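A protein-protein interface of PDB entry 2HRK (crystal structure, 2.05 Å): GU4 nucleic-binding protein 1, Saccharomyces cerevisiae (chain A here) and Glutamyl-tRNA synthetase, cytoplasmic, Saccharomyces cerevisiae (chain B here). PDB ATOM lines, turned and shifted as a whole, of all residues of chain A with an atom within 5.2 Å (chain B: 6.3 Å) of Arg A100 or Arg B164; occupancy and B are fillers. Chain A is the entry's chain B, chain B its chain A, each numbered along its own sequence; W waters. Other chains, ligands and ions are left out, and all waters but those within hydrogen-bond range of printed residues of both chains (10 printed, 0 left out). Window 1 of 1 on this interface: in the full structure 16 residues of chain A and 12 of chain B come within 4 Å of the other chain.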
ATOM      1  N   LEU A  51     -19.243   0.959 -10.330  1.00  0.00           N
ATOM      2  CA  LEU A  51     -18.474  -0.218 -10.681  1.00  0.00           C
ATOM      3  C   LEU A  51     -19.233  -1.536 -10.480  1.00  0.00           C
ATOM      4  O   LEU A  51     -18.853  -2.546 -11.046  1.00  0.00           O
ATOM      5  CB  LEU A  51     -17.151  -0.224  -9.911  1.00  0.00           C
ATOM      6  CG  LEU A  51     -16.172   0.869 -10.355  1.00  0.00           C
ATOM      7  CD1 LEU A  51     -14.982   0.988  -9.386  1.00  0.00           C
ATOM      8  CD2 LEU A  51     -15.694   0.609 -11.789  1.00  0.00           C
ATOM      9  N   ARG A  52     -20.299  -1.526  -9.680  1.00  0.00           N
ATOM     10  CA  ARG A  52     -21.186  -2.687  -9.568  1.00  0.00           C
ATOM     11  C   ARG A  52     -21.728  -3.132 -10.932  1.00  0.00           C
ATOM     12  O   ARG A  52     -21.814  -4.327 -11.212  1.00  0.00           O
ATOM     13  CB  ARG A  52     -22.365  -2.376  -8.644  1.00  0.00           C
ATOM     14  CG  ARG A  52     -23.304  -3.550  -8.417  1.00  0.00           C
ATOM     15  CD  ARG A  52     -24.594  -3.129  -7.728  1.00  0.00           C
ATOM     16  NE  ARG A  52     -25.456  -2.372  -8.633  1.00  0.00           N
ATOM     17  CZ  ARG A  52     -26.605  -1.793  -8.290  1.00  0.00           C
ATOM     18  NH1 ARG A  52     -27.062  -1.860  -7.046  1.00  0.00           N
ATOM     19  NH2 ARG A  52     -27.295  -1.124  -9.202  1.00  0.00           N
ATOM     20  N   ASP A  53     -22.102  -2.164 -11.760  1.00  0.00           N
ATOM     21  CA  ASP A  53     -22.751  -2.429 -13.039  1.00  0.00           C
ATOM     22  C   ASP A  53     -21.869  -2.141 -14.247  1.00  0.00           C
ATOM     23  O   ASP A  53     -22.255  -2.460 -15.366  1.00  0.00           O
ATOM     24  CB  ASP A  53     -23.998  -1.575 -13.169  1.00  0.00           C
ATOM     25  CG  ASP A  53     -25.005  -1.814 -12.059  1.00  0.00           C
ATOM     26  OD1 ASP A  53     -25.099  -2.942 -11.524  1.00  0.00           O
ATOM     27  OD2 ASP A  53     -25.730  -0.848 -11.750  1.00  0.00           O
ATOM     28  N   ASN A  54     -20.708  -1.526 -14.023  1.00  0.00           N
ATOM     29  CA  ASN A  54     -19.801  -1.133 -15.102  1.00  0.00           C
ATOM     30  C   ASN A  54     -18.386  -1.565 -14.788  1.00  0.00           C
ATOM     31  O   ASN A  54     -17.903  -1.341 -13.684  1.00  0.00           O
ATOM     32  CB  ASN A  54     -19.824   0.388 -15.285  1.00  0.00           C
ATOM     33  CG  ASN A  54     -21.210   0.912 -15.558  1.00  0.00           C
ATOM     34  OD1 ASN A  54     -21.706   0.817 -16.679  1.00  0.00           O
ATOM     35  ND2 ASN A  54     -21.854   1.447 -14.530  1.00  0.00           N
ATOM     36  N   THR A  55     -17.727  -2.181 -15.765  1.00  0.00           N
ATOM     37  CA  THR A  55     -16.358  -2.642 -15.601  1.00  0.00           C
ATOM     38  C   THR A  55     -15.420  -1.468 -15.348  1.00  0.00           C
ATOM     39  O   THR A  55     -14.591  -1.503 -14.436  1.00  0.00           O
ATOM     40  CB  THR A  55     -15.898  -3.429 -16.837  1.00  0.00           C
ATOM     41  OG1 THR A  55     -16.743  -4.574 -16.993  1.00  0.00           O
ATOM     42  CG2 THR A  55     -14.446  -3.880 -16.682  1.00  0.00           C
ATOM     43  N   PHE A  56     -15.568  -0.425 -16.164  1.00  0.00           N
ATOM     44  CA  PHE A  56     -14.789   0.796 -16.018  1.00  0.00           C
ATOM     45  C   PHE A  56     -15.732   1.970 -15.758  1.00  0.00           C
ATOM     46  O   PHE A  56     -16.933   1.887 -16.025  1.00  0.00           O
ATOM     47  CB  PHE A  56     -13.908   1.010 -17.250  1.00  0.00           C
ATOM     48  CG  PHE A  56     -13.037  -0.162 -17.557  1.00  0.00           C
ATOM     49  CD1 PHE A  56     -13.266  -0.950 -18.677  1.00  0.00           C
ATOM     50  CD2 PHE A  56     -12.013  -0.513 -16.691  1.00  0.00           C
ATOM     51  CE1 PHE A  56     -12.451  -2.047 -18.946  1.00  0.00           C
ATOM     52  CE2 PHE A  56     -11.206  -1.606 -16.951  1.00  0.00           C
ATOM     53  CZ  PHE A  56     -11.423  -2.374 -18.073  1.00  0.00           C
ATOM     54  N   ARG A  96     -16.350  -4.724  -3.031  1.00  0.00           N
ATOM     55  CA  ARG A  96     -15.726  -5.665  -3.949  1.00  0.00           C
ATOM     56  C   ARG A  96     -15.549  -5.097  -5.348  1.00  0.00           C
ATOM     57  O   ARG A  96     -14.630  -5.488  -6.056  1.00  0.00           O
ATOM     58  CB  ARG A  96     -16.523  -6.973  -4.035  1.00  0.00           C
ATOM     59  CG  ARG A  96     -17.941  -6.835  -4.560  1.00  0.00           C
ATOM     60  CD  ARG A  96     -18.512  -8.183  -4.933  1.00  0.00           C
ATOM     61  NE  ARG A  96     -18.440  -9.129  -3.819  1.00  0.00           N
ATOM     62  CZ  ARG A  96     -19.460  -9.850  -3.344  1.00  0.00           C
ATOM     63  NH1 ARG A  96     -20.681  -9.781  -3.885  1.00  0.00           N
ATOM     64  NH2 ARG A  96     -19.245 -10.673  -2.318  1.00  0.00           N
ATOM     65  N   HIS A  97     -16.435  -4.187  -5.742  1.00  0.00           N
ATOM     66  CA  HIS A  97     -16.438  -3.670  -7.108  1.00  0.00           C
ATOM     67  C   HIS A  97     -15.254  -2.734  -7.325  1.00  0.00           C
ATOM     68  O   HIS A  97     -14.570  -2.824  -8.339  1.00  0.00           O
ATOM     69  CB  HIS A  97     -17.782  -3.004  -7.427  1.00  0.00           C
ATOM     70  CG  HIS A  97     -18.954  -3.871  -7.087  1.00  0.00           C
ATOM     71  ND1 HIS A  97     -19.101  -5.144  -7.594  1.00  0.00           N
ATOM     72  CD2 HIS A  97     -20.007  -3.672  -6.258  1.00  0.00           C
ATOM     73  CE1 HIS A  97     -20.201  -5.686  -7.102  1.00  0.00           C
ATOM     74  NE2 HIS A  97     -20.769  -4.813  -6.289  1.00  0.00           N
ATOM     75  N   ILE A  98     -14.998  -1.865  -6.352  1.00  0.00           N
ATOM     76  CA  ILE A  98     -13.802  -1.028  -6.376  1.00  0.00           C
ATOM     77  C   ILE A  98     -12.568  -1.924  -6.352  1.00  0.00           C
ATOM     78  O   ILE A  98     -11.608  -1.675  -7.079  1.00  0.00           O
ATOM     79  CB  ILE A  98     -13.732  -0.048  -5.186  1.00  0.00           C
ATOM     80  CG1 ILE A  98     -14.905   0.942  -5.219  1.00  0.00           C
ATOM     81  CG2 ILE A  98     -12.407   0.725  -5.218  1.00  0.00           C
ATOM     82  CD1 ILE A  98     -14.867   1.968  -4.082  1.00  0.00           C
ATOM     83  N   LEU A  99     -12.619  -2.973  -5.534  1.00  0.00           N
ATOM     84  CA  LEU A  99     -11.505  -3.905  -5.383  1.00  0.00           C
ATOM     85  C   LEU A  99     -11.172  -4.657  -6.673  1.00  0.00           C
ATOM     86  O   LEU A  99     -10.007  -4.790  -7.019  1.00  0.00           O
ATOM     87  CB  LEU A  99     -11.779  -4.905  -4.250  1.00  0.00           C
ATOM     88  CG  LEU A  99     -11.611  -4.398  -2.816  1.00  0.00           C
ATOM     89  CD1 LEU A  99     -11.918  -5.512  -1.822  1.00  0.00           C
ATOM     90  CD2 LEU A  99     -10.214  -3.863  -2.609  1.00  0.00           C
ATOM     91  N   ARG A 100     -12.167  -5.153  -7.397  1.00  0.00           N
ATOM     92  CA  ARG A 100     -11.875  -5.806  -8.674  1.00  0.00           C
ATOM     93  C   ARG A 100     -11.348  -4.835  -9.725  1.00  0.00           C
ATOM     94  O   ARG A 100     -10.523  -5.188 -10.541  1.00  0.00           O
ATOM     95  CB  ARG A 100     -13.057  -6.620  -9.196  1.00  0.00           C
ATOM     96  CG  ARG A 100     -14.172  -5.833  -9.787  1.00  0.00           C
ATOM     97  CD  ARG A 100     -14.483  -6.134 -11.257  1.00  0.00           C
ATOM     98  NE  ARG A 100     -14.934  -4.929 -11.945  1.00  0.00           N
ATOM     99  CZ  ARG A 100     -15.999  -4.227 -11.604  1.00  0.00           C
ATOM    100  NH1 ARG A 100     -16.759  -4.622 -10.597  1.00  0.00           N
ATOM    101  NH2 ARG A 100     -16.312  -3.135 -12.270  1.00  0.00           N
ATOM    102  N   TRP A 101     -11.840  -3.609  -9.673  1.00  0.00           N
ATOM    103  CA  TRP A 101     -11.409  -2.546 -10.569  1.00  0.00           C
ATOM    104  C   TRP A 101      -9.992  -2.084 -10.209  1.00  0.00           C
ATOM    105  O   TRP A 101      -9.156  -1.899 -11.094  1.00  0.00           O
ATOM    106  CB  TRP A 101     -12.425  -1.394 -10.516  1.00  0.00           C
ATOM    107  CG  TRP A 101     -12.020  -0.108 -11.179  1.00  0.00           C
ATOM    108  CD1 TRP A 101     -12.097   0.205 -12.511  1.00  0.00           C
ATOM    109  CD2 TRP A 101     -11.518   1.051 -10.522  1.00  0.00           C
ATOM    110  NE1 TRP A 101     -11.651   1.485 -12.718  1.00  0.00           N
ATOM    111  CE2 TRP A 101     -11.296   2.030 -11.511  1.00  0.00           C
ATOM    112  CE3 TRP A 101     -11.229   1.359  -9.184  1.00  0.00           C
ATOM    113  CZ2 TRP A 101     -10.788   3.301 -11.206  1.00  0.00           C
ATOM    114  CZ3 TRP A 101     -10.731   2.626  -8.888  1.00  0.00           C
ATOM    115  CH2 TRP A 101     -10.518   3.576  -9.894  1.00  0.00           C
ATOM    116  N   ILE A 102      -9.723  -1.916  -8.916  1.00  0.00           N
ATOM    117  CA  ILE A 102      -8.355  -1.679  -8.443  1.00  0.00           C
ATOM    118  C   ILE A 102      -7.425  -2.767  -8.971  1.00  0.00           C
ATOM    119  O   ILE A 102      -6.386  -2.470  -9.531  1.00  0.00           O
ATOM    120  CB  ILE A 102      -8.251  -1.659  -6.893  1.00  0.00           C
ATOM    121  CG1 ILE A 102      -8.838  -0.370  -6.306  1.00  0.00           C
ATOM    122  CG2 ILE A 102      -6.786  -1.808  -6.434  1.00  0.00           C
ATOM    123  CD1 ILE A 102      -8.117   0.889  -6.701  1.00  0.00           C
ATOM    124  N   ASP A 103      -7.812  -4.029  -8.819  1.00  0.00           N
ATOM    125  CA  ASP A 103      -6.945  -5.138  -9.231  1.00  0.00           C
ATOM    126  C   ASP A 103      -6.645  -5.123 -10.727  1.00  0.00           C
ATOM    127  O   ASP A 103      -5.544  -5.477 -11.151  1.00  0.00           O
ATOM    128  CB  ASP A 103      -7.545  -6.486  -8.832  1.00  0.00           C
ATOM    129  CG  ASP A 103      -6.488  -7.603  -8.739  1.00  0.00           C
ATOM    130  OD1 ASP A 103      -5.285  -7.301  -8.566  1.00  0.00           O
ATOM    131  OD2 ASP A 103      -6.868  -8.784  -8.844  1.00  0.00           O
ATOM    132  N   TYR A 104      -7.623  -4.707 -11.528  1.00  0.00           N
ATOM    133  CA  TYR A 104      -7.412  -4.589 -12.965  1.00  0.00           C
ATOM    134  C   TYR A 104      -6.437  -3.457 -13.290  1.00  0.00           C
ATOM    135  O   TYR A 104      -5.477  -3.646 -14.034  1.00  0.00           O
ATOM    136  CB  TYR A 104      -8.729  -4.350 -13.693  1.00  0.00           C
ATOM    137  CG  TYR A 104      -8.570  -4.485 -15.181  1.00  0.00           C
ATOM    138  CD1 TYR A 104      -8.760  -5.714 -15.805  1.00  0.00           C
ATOM    139  CD2 TYR A 104      -8.180  -3.400 -15.963  1.00  0.00           C
ATOM    140  CE1 TYR A 104      -8.593  -5.851 -17.165  1.00  0.00           C
ATOM    141  CE2 TYR A 104      -8.023  -3.529 -17.330  1.00  0.00           C
ATOM    142  CZ  TYR A 104      -8.229  -4.756 -17.919  1.00  0.00           C
ATOM    143  OH  TYR A 104      -8.062  -4.911 -19.267  1.00  0.00           O
ATOM    144  N   LEU B 121     -16.996 -14.000 -10.533  1.00  0.00           N
ATOM    145  CA  LEU B 121     -16.716 -12.639 -10.996  1.00  0.00           C
ATOM    146  C   LEU B 121     -16.651 -11.571  -9.890  1.00  0.00           C
ATOM    147  O   LEU B 121     -16.363 -10.411 -10.189  1.00  0.00           O
ATOM    148  CB  LEU B 121     -17.742 -12.228 -12.073  1.00  0.00           C
ATOM    149  CG  LEU B 121     -17.632 -12.928 -13.441  1.00  0.00           C
ATOM    150  CD1 LEU B 121     -18.887 -12.697 -14.291  1.00  0.00           C
ATOM    151  CD2 LEU B 121     -16.382 -12.487 -14.221  1.00  0.00           C
ATOM    152  N   ASN B 122     -16.897 -11.940  -8.627  1.00  0.00           N
ATOM    153  CA  ASN B 122     -16.881 -10.961  -7.515  1.00  0.00           C
ATOM    154  C   ASN B 122     -15.725  -9.966  -7.629  1.00  0.00           C
ATOM    155  O   ASN B 122     -15.934  -8.749  -7.576  1.00  0.00           O
ATOM    156  CB  ASN B 122     -16.784 -11.659  -6.145  1.00  0.00           C
ATOM    157  CG  ASN B 122     -18.127 -12.185  -5.633  1.00  0.00           C
ATOM    158  OD1 ASN B 122     -18.160 -13.097  -4.804  1.00  0.00           O
ATOM    159  ND2 ASN B 122     -19.223 -11.600  -6.094  1.00  0.00           N
ATOM    160  N   LEU B 123     -14.518 -10.500  -7.790  1.00  0.00           N
ATOM    161  CA  LEU B 123     -13.288  -9.692  -7.791  1.00  0.00           C
ATOM    162  C   LEU B 123     -12.496  -9.802  -9.092  1.00  0.00           C
ATOM    163  O   LEU B 123     -11.298  -9.495  -9.116  1.00  0.00           O
ATOM    164  CB  LEU B 123     -12.375 -10.090  -6.621  1.00  0.00           C
ATOM    165  CG  LEU B 123     -12.914  -9.849  -5.219  1.00  0.00           C
ATOM    166  CD1 LEU B 123     -11.968 -10.501  -4.201  1.00  0.00           C
ATOM    167  CD2 LEU B 123     -13.084  -8.372  -4.940  1.00  0.00           C
ATOM    168  N   ARG B 124     -13.175 -10.204 -10.170  1.00  0.00           N
ATOM    169  CA  ARG B 124     -12.547 -10.416 -11.467  1.00  0.00           C
ATOM    170  C   ARG B 124     -13.300  -9.698 -12.589  1.00  0.00           C
ATOM    171  O   ARG B 124     -14.526  -9.598 -12.563  1.00  0.00           O
ATOM    172  CB  ARG B 124     -12.478 -11.910 -11.777  1.00  0.00           C
ATOM    173  CG  ARG B 124     -11.727 -12.735 -10.748  1.00  0.00           C
ATOM    174  CD  ARG B 124     -11.629 -14.183 -11.190  1.00  0.00           C
ATOM    175  NE  ARG B 124     -10.718 -14.963 -10.357  1.00  0.00           N
ATOM    176  CZ  ARG B 124     -11.064 -15.639  -9.258  1.00  0.00           C
ATOM    177  NH1 ARG B 124     -12.325 -15.674  -8.827  1.00  0.00           N
ATOM    178  NH2 ARG B 124     -10.132 -16.309  -8.584  1.00  0.00           N
ATOM    179  N   THR B 125     -12.551  -9.199 -13.569  1.00  0.00           N
ATOM    180  CA  THR B 125     -13.119  -8.563 -14.763  1.00  0.00           C
ATOM    181  C   THR B 125     -13.486  -9.621 -15.811  1.00  0.00           C
ATOM    182  O   THR B 125     -14.469  -9.481 -16.560  1.00  0.00           O
ATOM    183  CB  THR B 125     -12.104  -7.550 -15.357  1.00  0.00           C
ATOM    184  OG1 THR B 125     -11.888  -6.497 -14.416  1.00  0.00           O
ATOM    185  CG2 THR B 125     -12.594  -6.940 -16.669  1.00  0.00           C
ATOM    186  N   PHE B 126     -12.669 -10.671 -15.868  1.00  0.00           N
ATOM    187  CA  PHE B 126     -12.937 -11.836 -16.705  1.00  0.00           C
ATOM    188  C   PHE B 126     -12.935 -13.089 -15.848  1.00  0.00           C
ATOM    189  O   PHE B 126     -12.402 -13.093 -14.730  1.00  0.00           O
ATOM    190  CB  PHE B 126     -11.910 -11.935 -17.824  1.00  0.00           C
ATOM    191  CG  PHE B 126     -11.841 -10.705 -18.678  1.00  0.00           C
ATOM    192  CD1 PHE B 126     -10.762  -9.829 -18.579  1.00  0.00           C
ATOM    193  CD2 PHE B 126     -12.864 -10.402 -19.562  1.00  0.00           C
ATOM    194  CE1 PHE B 126     -10.706  -8.677 -19.363  1.00  0.00           C
ATOM    195  CE2 PHE B 126     -12.812  -9.262 -20.348  1.00  0.00           C
ATOM    196  CZ  PHE B 126     -11.730  -8.396 -20.244  1.00  0.00           C
ATOM    197  N   ASP B 159     -28.015 -10.757 -11.010  1.00  0.00           N
ATOM    198  CA  ASP B 159     -26.647 -11.194 -10.774  1.00  0.00           C
ATOM    199  C   ASP B 159     -25.769 -10.078 -11.316  1.00  0.00           C
ATOM    200  O   ASP B 159     -25.423 -10.065 -12.498  1.00  0.00           O
ATOM    201  CB  ASP B 159     -26.368 -12.529 -11.483  1.00  0.00           C
ATOM    202  CG  ASP B 159     -27.075 -13.713 -10.820  1.00  0.00           C
ATOM    203  OD1 ASP B 159     -27.041 -13.831  -9.579  1.00  0.00           O
ATOM    204  OD2 ASP B 159     -27.652 -14.548 -11.541  1.00  0.00           O
ATOM    205  N   VAL B 160     -25.446  -9.125 -10.442  1.00  0.00           N
ATOM    206  CA  VAL B 160     -24.812  -7.869 -10.839  1.00  0.00           C
ATOM    207  C   VAL B 160     -23.486  -8.072 -11.562  1.00  0.00           C
ATOM    208  O   VAL B 160     -23.213  -7.372 -12.522  1.00  0.00           O
ATOM    209  CB  VAL B 160     -24.607  -6.891  -9.641  1.00  0.00           C
ATOM    210  CG1 VAL B 160     -25.962  -6.430  -9.083  1.00  0.00           C
ATOM    211  CG2 VAL B 160     -23.766  -7.522  -8.554  1.00  0.00           C
ATOM    212  N   ASN B 161     -22.675  -9.022 -11.103  1.00  0.00           N
ATOM    213  CA  ASN B 161     -21.376  -9.279 -11.726  1.00  0.00           C
ATOM    214  C   ASN B 161     -21.541  -9.849 -13.136  1.00  0.00           C
ATOM    215  O   ASN B 161     -20.855  -9.438 -14.064  1.00  0.00           O
ATOM    216  CB  ASN B 161     -20.529 -10.215 -10.858  1.00  0.00           C
ATOM    217  CG  ASN B 161     -20.378  -9.714  -9.416  1.00  0.00           C
ATOM    218  OD1 ASN B 161     -20.431  -8.513  -9.156  1.00  0.00           O
ATOM    219  ND2 ASN B 161     -20.187 -10.638  -8.486  1.00  0.00           N
ATOM    220  N   VAL B 162     -22.482 -10.778 -13.289  1.00  0.00           N
ATOM    221  CA  VAL B 162     -22.788 -11.365 -14.592  1.00  0.00           C
ATOM    222  C   VAL B 162     -23.246 -10.288 -15.580  1.00  0.00           C
ATOM    223  O   VAL B 162     -22.758 -10.233 -16.713  1.00  0.00           O
ATOM    224  CB  VAL B 162     -23.846 -12.495 -14.464  1.00  0.00           C
ATOM    225  CG1 VAL B 162     -24.286 -12.998 -15.855  1.00  0.00           C
ATOM    226  CG2 VAL B 162     -23.285 -13.644 -13.641  1.00  0.00           C
ATOM    227  N   SER B 163     -24.145  -9.406 -15.150  1.00  0.00           N
ATOM    228  CA  SER B 163     -24.616  -8.321 -16.024  1.00  0.00           C
ATOM    229  C   SER B 163     -23.477  -7.358 -16.396  1.00  0.00           C
ATOM    230  O   SER B 163     -23.321  -6.967 -17.549  1.00  0.00           O
ATOM    231  CB  SER B 163     -25.782  -7.569 -15.369  1.00  0.00           C
ATOM    232  OG  SER B 163     -26.941  -8.392 -15.324  1.00  0.00           O
ATOM    233  N   ARG B 164     -22.675  -6.992 -15.406  1.00  0.00           N
ATOM    234  CA  ARG B 164     -21.510  -6.134 -15.618  1.00  0.00           C
ATOM    235  C   ARG B 164     -20.523  -6.754 -16.617  1.00  0.00           C
ATOM    236  O   ARG B 164     -20.025  -6.081 -17.523  1.00  0.00           O
ATOM    237  CB  ARG B 164     -20.845  -5.910 -14.268  1.00  0.00           C
ATOM    238  CG  ARG B 164     -19.600  -5.063 -14.262  1.00  0.00           C
ATOM    239  CD  ARG B 164     -18.647  -5.623 -13.234  1.00  0.00           C
ATOM    240  NE  ARG B 164     -17.902  -6.737 -13.783  1.00  0.00           N
ATOM    241  CZ  ARG B 164     -17.438  -7.795 -13.121  1.00  0.00           C
ATOM    242  NH1 ARG B 164     -17.660  -7.991 -11.826  1.00  0.00           N
ATOM    243  NH2 ARG B 164     -16.759  -8.703 -13.805  1.00  0.00           N
ATOM    244  N   TRP B 165     -20.271  -8.046 -16.455  1.00  0.00           N
ATOM    245  CA  TRP B 165     -19.357  -8.784 -17.323  1.00  0.00           C
ATOM    246  C   TRP B 165     -19.952  -8.973 -18.718  1.00  0.00           C
ATOM    247  O   TRP B 165     -19.287  -8.725 -19.736  1.00  0.00           O
ATOM    248  CB  TRP B 165     -19.002 -10.126 -16.664  1.00  0.00           C
ATOM    249  CG  TRP B 165     -18.441 -11.145 -17.583  1.00  0.00           C
ATOM    250  CD1 TRP B 165     -17.146 -11.278 -17.967  1.00  0.00           C
ATOM    251  CD2 TRP B 165     -19.164 -12.193 -18.234  1.00  0.00           C
ATOM    252  NE1 TRP B 165     -17.012 -12.337 -18.836  1.00  0.00           N
ATOM    253  CE2 TRP B 165     -18.240 -12.917 -19.016  1.00  0.00           C
ATOM    254  CE3 TRP B 165     -20.505 -12.586 -18.240  1.00  0.00           C
ATOM    255  CZ2 TRP B 165     -18.613 -14.021 -19.784  1.00  0.00           C
ATOM    256  CZ3 TRP B 165     -20.874 -13.678 -19.013  1.00  0.00           C
ATOM    257  CH2 TRP B 165     -19.933 -14.382 -19.767  1.00  0.00           C
ATOM    258  N   TYR B 166     -21.214  -9.382 -18.765  1.00  0.00           N
ATOM    259  CA  TYR B 166     -21.877  -9.658 -20.035  1.00  0.00           C
ATOM    260  C   TYR B 166     -21.956  -8.392 -20.896  1.00  0.00           C
ATOM    261  O   TYR B 166     -21.637  -8.420 -22.093  1.00  0.00           O
ATOM    262  CB  TYR B 166     -23.267 -10.257 -19.802  1.00  0.00           C
ATOM    263  CG  TYR B 166     -23.976 -10.651 -21.086  1.00  0.00           C
ATOM    264  CD1 TYR B 166     -23.932 -11.958 -21.556  1.00  0.00           C
ATOM    265  CD2 TYR B 166     -24.688  -9.708 -21.828  1.00  0.00           C
ATOM    266  CE1 TYR B 166     -24.578 -12.316 -22.737  1.00  0.00           C
ATOM    267  CE2 TYR B 166     -25.332 -10.058 -23.003  1.00  0.00           C
ATOM    268  CZ  TYR B 166     -25.274 -11.356 -23.453  1.00  0.00           C
ATOM    269  OH  TYR B 166     -25.914 -11.692 -24.624  1.00  0.00           O
ATOM    270  N   THR B 167     -22.344  -7.273 -20.290  1.00  0.00           N
ATOM    271  CA  THR B 167     -22.462  -6.026 -21.036  1.00  0.00           C
ATOM    272  C   THR B 167     -21.112  -5.452 -21.486  1.00  0.00           C
ATOM    273  O   THR B 167     -21.054  -4.681 -22.446  1.00  0.00           O
ATOM    274  CB  THR B 167     -23.279  -4.962 -20.271  1.00  0.00           C
ATOM    275  OG1 THR B 167     -22.630  -4.639 -19.036  1.00  0.00           O
ATOM    276  CG2 THR B 167     -24.689  -5.480 -20.001  1.00  0.00           C
ATOM    277  N   LEU B 168     -20.028  -5.832 -20.815  1.00  0.00           N
ATOM    278  CA  LEU B 168     -18.696  -5.447 -21.270  1.00  0.00           C
ATOM    279  C   LEU B 168     -18.403  -6.093 -22.626  1.00  0.00           C
ATOM    280  O   LEU B 168     -18.115  -5.407 -23.607  1.00  0.00           O
ATOM    281  CB  LEU B 168     -17.632  -5.857 -20.254  1.00  0.00           C
ATOM    282  CG  LEU B 168     -16.169  -5.586 -20.639  1.00  0.00           C
ATOM    283  CD1 LEU B 168     -15.871  -4.084 -20.670  1.00  0.00           C
ATOM    284  CD2 LEU B 168     -15.250  -6.330 -19.685  1.00  0.00           C
ATOM    285  N   LEU B 169     -18.487  -7.417 -22.670  1.00  0.00           N
ATOM    286  CA  LEU B 169     -18.127  -8.162 -23.880  1.00  0.00           C
ATOM    287  C   LEU B 169     -19.078  -7.839 -25.042  1.00  0.00           C
ATOM    288  O   LEU B 169     -18.667  -7.786 -26.191  1.00  0.00           O
ATOM    289  CB  LEU B 169     -18.078  -9.664 -23.583  1.00  0.00           C
ATOM    290  CG  LEU B 169     -16.980 -10.087 -22.593  1.00  0.00           C
ATOM    291  CD1 LEU B 169     -17.090 -11.557 -22.241  1.00  0.00           C
ATOM    292  CD2 LEU B 169     -15.614  -9.778 -23.162  1.00  0.00           C
HETATM  293  O   HOH W   1     -16.235  -7.444 -16.460  1.00  0.00           O
HETATM  294  O   HOH W   2     -20.004  -6.268 -10.732  1.00  0.00           O
HETATM  295  O   HOH W   3      -8.970  -9.553 -10.057  1.00  0.00           O
HETATM  296  O   HOH W   4     -24.403  -4.119 -15.537  1.00  0.00           O
HETATM  297  O   HOH W   5     -10.333  -7.262 -12.219  1.00  0.00           O
HETATM  298  O   HOH W   6     -24.738  -5.120 -12.972  1.00  0.00           O
HETATM  299  O   HOH W   7     -19.264  -3.446 -18.079  1.00  0.00           O
HETATM  300  O   HOH W   8     -21.926  -8.524  -6.566  1.00  0.00           O
HETATM  301  O   HOH W   9     -17.514  -6.943  -8.915  1.00  0.00           O
HETATM  302  O   HOH W  10     -13.066  -3.710 -13.558  1.00  0.00           O
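The side-chain amide nitrogen (ND2) of Asn B122 lies close to the guanidinium group (NH1) of Arg A96, 3.2 Å away.
Water W3 bridges O of Leu B123 and OD2 of Asp A103. Water W6 lies within hydrogen-bond range of OD1 of Asp A53 and O of Val B160. Water W5 lies within hydrogen-bond range of the backbone carbonyl oxygen (O) of Arg A100 (2.7 Å) and the side-chain hydroxyl (OG1) of Thr B125 (2.8 Å). Water W1 lies within hydrogen-bond range of O of Thr B125 (2.7 Å), OG1 of Thr A55 (3.0 Å) and NH2 of Arg B164 (3.0 Å). Water W7 lies within hydrogen-bond range of the backbone carbonyl oxygen (O) of Arg B164 (2.8 Å) and the side-chain hydroxyl (OG1) of Thr A55 (3.0 Å). Water W8 lies within hydrogen-bond range of OD1 of Asn B161 (3.0 Å) and NH1 of Arg A96 (3.2 Å).
O of Leu A51 lies within hydrogen-bond range of NH2 of Arg A100. The backbone carbonyl oxygen (O) of Arg B164 is in hydrogen-bond range of the side-chain hydroxyl (OG1) of Thr B167 (3.3 Å). The backbone carbonyl oxygen of Arg B124 lies within hydrogen-bond range of the guanidinium group of Arg B164. The side-chain amide nitrogen (ND2) of Asn B122 sits close to the side-chain amide nitrogen (ND2) of Asn B161 (2.8 Å). The side-chain carboxylate (OD1) of Asp A53 lies within salt-bridge range of the guanidinium group (NE) of Arg A52 (3.0 Å). NH2 of Arg A100 is in hydrogen-bond range of O of Asn A54 (2.8 Å).
CG of Arg B164 touches C of Asp A53, at 3.7 Å. CG of Arg B164 touches N of Asn A54 (3.7 Å). CG2 of Thr B125 touches CG2 of Thr A55 (3.6 Å). Thr A55 touches Leu B168. His A97 touches Asn B161 (CE1 to OD1, 3.5 Å). Leu A99 touches Leu B123. Arg A100 touches Leu B123. Arg B124 touches Arg A100 (O to CD, 3.7 Å). Arg A100 touches Arg B164 (NH1 to CD, 3.4 Å). OG1 of Thr B125 touches CD1 of Tyr A104, at 3.5 Å.
Of the printed residues of chain B, Asn A54 touches Arg B164. Of the printed residues of chain B, Thr A55 touches Thr B125, Arg B164 and Leu B168. Of chain B, only Asn B122, Leu B123, Arg B124 and Arg B164 come within 4 Å of Arg A100. Trp A101 touches none of the printed residues of chain B. Of the printed residues of chain B, Tyr A104 touches Thr B125 (3.5 Å). Leu B121 touches none of the printed residues of chain A. Of the printed residues of chain A, Asn B161 touches His A97 (3.5 Å). The nearest residue of chain B that does not touch Arg A100 is Thr B125 (4.1 Å). The nearest printed residue of chain A that does not touch Thr B125 is Arg A100 (4.1 Å).
Of the 17 printed residues of chain B, 8 touch a printed residue of chain A. Printed residues of chain A that touch a printed residue of chain B: Leu A51, Arg A52, Asp A53, Asn A54, Thr A55, Arg A96, His A97, Leu A99, Arg A100 and Tyr A104.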
